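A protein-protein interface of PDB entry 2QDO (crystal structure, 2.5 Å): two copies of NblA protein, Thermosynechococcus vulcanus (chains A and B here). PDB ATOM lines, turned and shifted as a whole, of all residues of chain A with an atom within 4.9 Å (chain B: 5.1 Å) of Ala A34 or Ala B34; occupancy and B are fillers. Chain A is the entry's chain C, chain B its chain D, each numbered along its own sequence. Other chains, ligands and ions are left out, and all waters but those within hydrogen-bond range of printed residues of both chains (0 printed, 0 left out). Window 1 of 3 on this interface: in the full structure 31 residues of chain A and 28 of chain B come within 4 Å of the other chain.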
ATOM      1  N   LEU A  30      23.087   4.862  11.794  1.00  0.00           N
ATOM      2  CA  LEU A  30      24.304   5.627  12.087  1.00  0.00           C
ATOM      3  C   LEU A  30      24.285   7.047  11.512  1.00  0.00           C
ATOM      4  O   LEU A  30      24.673   7.981  12.201  1.00  0.00           O
ATOM      5  CB  LEU A  30      25.557   4.882  11.589  1.00  0.00           C
ATOM      6  CG  LEU A  30      25.928   3.551  12.261  1.00  0.00           C
ATOM      7  CD1 LEU A  30      27.349   3.197  11.901  1.00  0.00           C
ATOM      8  CD2 LEU A  30      25.812   3.654  13.795  1.00  0.00           C
ATOM      9  N   LEU A  31      23.837   7.207  10.264  1.00  0.00           N
ATOM     10  CA  LEU A  31      23.772   8.520   9.611  1.00  0.00           C
ATOM     11  C   LEU A  31      22.871   9.439  10.437  1.00  0.00           C
ATOM     12  O   LEU A  31      23.145  10.631  10.602  1.00  0.00           O
ATOM     13  CB  LEU A  31      23.171   8.391   8.210  1.00  0.00           C
ATOM     14  CG  LEU A  31      23.547   9.334   7.056  1.00  0.00           C
ATOM     15  CD1 LEU A  31      22.376   9.354   6.071  1.00  0.00           C
ATOM     16  CD2 LEU A  31      23.843  10.760   7.548  1.00  0.00           C
ATOM     17  N   LEU A  32      21.774   8.872  10.927  1.00  0.00           N
ATOM     18  CA  LEU A  32      20.822   9.616  11.736  1.00  0.00           C
ATOM     19  C   LEU A  32      21.469   9.967  13.056  1.00  0.00           C
ATOM     20  O   LEU A  32      21.246  11.051  13.593  1.00  0.00           O
ATOM     21  CB  LEU A  32      19.565   8.780  11.977  1.00  0.00           C
ATOM     22  CG  LEU A  32      18.280   9.290  11.329  1.00  0.00           C
ATOM     23  CD1 LEU A  32      18.591   9.852   9.970  1.00  0.00           C
ATOM     24  CD2 LEU A  32      17.274   8.155  11.224  1.00  0.00           C
ATOM     25  N   GLN A  33      22.258   9.040  13.588  1.00  0.00           N
ATOM     26  CA  GLN A  33      22.942   9.307  14.840  1.00  0.00           C
ATOM     27  C   GLN A  33      23.986  10.393  14.584  1.00  0.00           C
ATOM     28  O   GLN A  33      24.242  11.220  15.449  1.00  0.00           O
ATOM     29  CB  GLN A  33      23.593   8.037  15.403  1.00  0.00           C
ATOM     30  CG  GLN A  33      22.605   7.139  16.148  1.00  0.00           C
ATOM     31  CD  GLN A  33      23.246   5.902  16.763  1.00  0.00           C
ATOM     32  OE1 GLN A  33      22.665   4.817  16.731  1.00  0.00           O
ATOM     33  NE2 GLN A  33      24.439   6.061  17.335  1.00  0.00           N
ATOM     34  N   ALA A  34      24.546  10.409  13.377  1.00  0.00           N
ATOM     35  CA  ALA A  34      25.543  11.406  13.003  1.00  0.00           C
ATOM     36  C   ALA A  34      24.946  12.814  12.792  1.00  0.00           C
ATOM     37  O   ALA A  34      25.526  13.808  13.234  1.00  0.00           O
ATOM     38  CB  ALA A  34      26.287  10.948  11.736  1.00  0.00           C
ATOM     39  N   SER A  35      23.804  12.892  12.106  1.00  0.00           N
ATOM     40  CA  SER A  35      23.135  14.171  11.837  1.00  0.00           C
ATOM     41  C   SER A  35      22.677  14.831  13.134  1.00  0.00           C
ATOM     42  O   SER A  35      22.749  16.046  13.284  1.00  0.00           O
ATOM     43  CB  SER A  35      21.936  13.948  10.921  1.00  0.00           C
ATOM     44  OG  SER A  35      22.350  13.286   9.743  1.00  0.00           O
ATOM     45  N   ARG A  36      22.187  14.024  14.061  1.00  0.00           N
ATOM     46  CA  ARG A  36      21.767  14.534  15.355  1.00  0.00           C
ATOM     47  C   ARG A  36      23.009  15.092  16.064  1.00  0.00           C
ATOM     48  O   ARG A  36      22.998  16.207  16.583  1.00  0.00           O
ATOM     49  CB  ARG A  36      21.146  13.402  16.181  1.00  0.00           C
ATOM     50  CG  ARG A  36      20.860  13.737  17.642  1.00  0.00           C
ATOM     51  CD  ARG A  36      20.255  12.531  18.339  1.00  0.00           C
ATOM     52  NE  ARG A  36      18.896  12.262  17.883  1.00  0.00           N
ATOM     53  CZ  ARG A  36      17.827  12.923  18.317  1.00  0.00           C
ATOM     54  NH1 ARG A  36      17.969  13.882  19.224  1.00  0.00           N
ATOM     55  NH2 ARG A  36      16.623  12.644  17.832  1.00  0.00           N
ATOM     56  N   LEU A  37      24.084  14.315  16.050  1.00  0.00           N
ATOM     57  CA  LEU A  37      25.334  14.713  16.691  1.00  0.00           C
ATOM     58  C   LEU A  37      25.891  15.991  16.047  1.00  0.00           C
ATOM     59  O   LEU A  37      26.528  16.805  16.705  1.00  0.00           O
ATOM     60  CB  LEU A  37      26.360  13.580  16.587  1.00  0.00           C
ATOM     61  CG  LEU A  37      27.536  13.580  17.565  1.00  0.00           C
ATOM     62  CD1 LEU A  37      27.060  13.959  18.960  1.00  0.00           C
ATOM     63  CD2 LEU A  37      28.178  12.188  17.568  1.00  0.00           C
ATOM     64  N   LEU A  38      25.672  16.172  14.753  1.00  0.00           N
ATOM     65  CA  LEU A  38      26.164  17.382  14.119  1.00  0.00           C
ATOM     66  C   LEU A  38      25.468  18.595  14.751  1.00  0.00           C
ATOM     67  O   LEU A  38      26.109  19.598  15.043  1.00  0.00           O
ATOM     68  CB  LEU A  38      25.912  17.346  12.604  1.00  0.00           C
ATOM     69  CG  LEU A  38      26.921  16.517  11.786  1.00  0.00           C
ATOM     70  CD1 LEU A  38      26.405  16.359  10.354  1.00  0.00           C
ATOM     71  CD2 LEU A  38      28.316  17.199  11.802  1.00  0.00           C
ATOM     72  N   LEU B  30      27.070  10.035   2.324  1.00  0.00           N
ATOM     73  CA  LEU B  30      26.666  10.981   3.350  1.00  0.00           C
ATOM     74  C   LEU B  30      27.082  10.637   4.781  1.00  0.00           C
ATOM     75  O   LEU B  30      27.259  11.539   5.602  1.00  0.00           O
ATOM     76  CB  LEU B  30      25.154  11.170   3.285  1.00  0.00           C
ATOM     77  CG  LEU B  30      24.606  12.472   2.689  1.00  0.00           C
ATOM     78  CD1 LEU B  30      25.416  12.927   1.480  1.00  0.00           C
ATOM     79  CD2 LEU B  30      23.144  12.246   2.315  1.00  0.00           C
ATOM     80  N   LEU B  31      27.233   9.356   5.095  1.00  0.00           N
ATOM     81  CA  LEU B  31      27.644   8.964   6.448  1.00  0.00           C
ATOM     82  C   LEU B  31      29.096   9.399   6.597  1.00  0.00           C
ATOM     83  O   LEU B  31      29.536   9.764   7.687  1.00  0.00           O
ATOM     84  CB  LEU B  31      27.590   7.444   6.638  1.00  0.00           C
ATOM     85  CG  LEU B  31      27.247   6.796   7.987  1.00  0.00           C
ATOM     86  CD1 LEU B  31      27.899   5.413   8.006  1.00  0.00           C
ATOM     87  CD2 LEU B  31      27.747   7.609   9.171  1.00  0.00           C
ATOM     88  N   LEU B  32      29.841   9.319   5.495  1.00  0.00           N
ATOM     89  CA  LEU B  32      31.250   9.705   5.494  1.00  0.00           C
ATOM     90  C   LEU B  32      31.369  11.187   5.649  1.00  0.00           C
ATOM     91  O   LEU B  32      32.092  11.664   6.519  1.00  0.00           O
ATOM     92  CB  LEU B  32      31.951   9.291   4.202  1.00  0.00           C
ATOM     93  CG  LEU B  32      32.343   7.820   4.180  1.00  0.00           C
ATOM     94  CD1 LEU B  32      33.403   7.573   3.118  1.00  0.00           C
ATOM     95  CD2 LEU B  32      32.854   7.436   5.557  1.00  0.00           C
ATOM     96  N   GLN B  33      30.651  11.909   4.798  1.00  0.00           N
ATOM     97  CA  GLN B  33      30.679  13.349   4.863  1.00  0.00           C
ATOM     98  C   GLN B  33      30.391  13.827   6.275  1.00  0.00           C
ATOM     99  O   GLN B  33      31.095  14.693   6.783  1.00  0.00           O
ATOM    100  CB  GLN B  33      29.665  13.959   3.904  1.00  0.00           C
ATOM    101  CG  GLN B  33      29.562  15.455   4.074  1.00  0.00           C
ATOM    102  CD  GLN B  33      28.743  16.110   3.001  1.00  0.00           C
ATOM    103  OE1 GLN B  33      28.995  15.914   1.816  1.00  0.00           O
ATOM    104  NE2 GLN B  33      27.756  16.907   3.405  1.00  0.00           N
ATOM    105  N   ALA B  34      29.363  13.264   6.901  1.00  0.00           N
ATOM    106  CA  ALA B  34      28.997  13.668   8.254  1.00  0.00           C
ATOM    107  C   ALA B  34      30.093  13.343   9.244  1.00  0.00           C
ATOM    108  O   ALA B  34      30.228  14.008  10.267  1.00  0.00           O
ATOM    109  CB  ALA B  34      27.687  13.005   8.684  1.00  0.00           C
ATOM    110  N   SER B  35      30.871  12.316   8.945  1.00  0.00           N
ATOM    111  CA  SER B  35      31.966  11.937   9.824  1.00  0.00           C
ATOM    112  C   SER B  35      33.110  12.947   9.704  1.00  0.00           C
ATOM    113  O   SER B  35      33.750  13.289  10.704  1.00  0.00           O
ATOM    114  CB  SER B  35      32.462  10.536   9.472  1.00  0.00           C
ATOM    115  OG  SER B  35      31.462   9.569   9.740  1.00  0.00           O
ATOM    116  N   ARG B  36      33.356  13.404   8.480  1.00  0.00           N
ATOM    117  CA  ARG B  36      34.387  14.396   8.226  1.00  0.00           C
ATOM    118  C   ARG B  36      33.966  15.626   9.044  1.00  0.00           C
ATOM    119  O   ARG B  36      34.705  16.084   9.926  1.00  0.00           O
ATOM    120  CB  ARG B  36      34.456  14.712   6.717  1.00  0.00           C
ATOM    121  CG  ARG B  36      35.359  15.884   6.322  1.00  0.00           C
ATOM    122  CD  ARG B  36      35.436  16.042   4.810  1.00  0.00           C
ATOM    123  NE  ARG B  36      36.046  14.875   4.186  1.00  0.00           N
ATOM    124  CZ  ARG B  36      37.342  14.588   4.243  1.00  0.00           C
ATOM    125  NH1 ARG B  36      38.166  15.394   4.890  1.00  0.00           N
ATOM    126  NH2 ARG B  36      37.810  13.482   3.675  1.00  0.00           N
ATOM    127  N   LEU B  37      32.758  16.119   8.775  1.00  0.00           N
ATOM    128  CA  LEU B  37      32.201  17.276   9.474  1.00  0.00           C
ATOM    129  C   LEU B  37      32.276  17.215  11.000  1.00  0.00           C
ATOM    130  O   LEU B  37      32.552  18.218  11.649  1.00  0.00           O
ATOM    131  CB  LEU B  37      30.743  17.482   9.062  1.00  0.00           C
ATOM    132  CG  LEU B  37      30.577  18.294   7.783  1.00  0.00           C
ATOM    133  CD1 LEU B  37      29.109  18.430   7.437  1.00  0.00           C
ATOM    134  CD2 LEU B  37      31.217  19.665   7.987  1.00  0.00           C
ATOM    135  N   LEU B  38      31.991  16.057  11.580  1.00  0.00           N
ATOM    136  CA  LEU B  38      32.050  15.932  13.026  1.00  0.00           C
ATOM    137  C   LEU B  38      33.466  16.184  13.497  1.00  0.00           C
ATOM    138  O   LEU B  38      33.692  16.726  14.573  1.00  0.00           O
ATOM    139  CB  LEU B  38      31.617  14.540  13.467  1.00  0.00           C
ATOM    140  CG  LEU B  38      30.158  14.199  13.176  1.00  0.00           C
ATOM    141  CD1 LEU B  38      29.920  12.740  13.538  1.00  0.00           C
ATOM    142  CD2 LEU B  38      29.229  15.125  13.979  1.00  0.00           C
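Of the printed residues of chain B, Ala A34 touches Ala B34 (3.9 Å). Ala B34 touches two residues of chain A. Of the printed residues of chain A, Leu B38 touches Leu A38. Of the printed residues of chain A, Leu B37 touches Leu A38 (3.7 Å). Of the printed residues of chain B, Leu A38 touches Ala B34 (3.96 Å), Leu B37 (3.7 Å) and Leu B38 (3.1 Å). Arg A36 touches none of the printed residues of chain B. Leu B30 touches none of the printed residues of chain A. The nearest residue of chain A that does not touch Ala B34 is Leu A31 (4.6 Å).
CB of Ala A34 touches CB of Ala B34, 3.9 Å away. Leu A38 touches Ala B34. CD2 of Leu A38 touches CB of Leu B37, at 3.7 Å. CD2 of Leu A38 touches CD2 of Leu B38 (3.1 Å).
Ala A34 touches its own counterpart, Ala B34. Leu A38 touches Ala B34, but with the chains exchanged Ala A34 does not touch Leu B38 (4.0002 Å). Leu A38 touches Leu B37, but with the chains exchanged Leu A37 does not touch Leu B38 (4.02 Å). Leu A38 touches its own counterpart, Leu B38. 9 positions are printed for both chains.
Printed residues of chain B that touch a printed residue of chain A: Ala B34, Leu B37 and Leu B38. Among the printed residues, 4 pairs touch across the chains.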
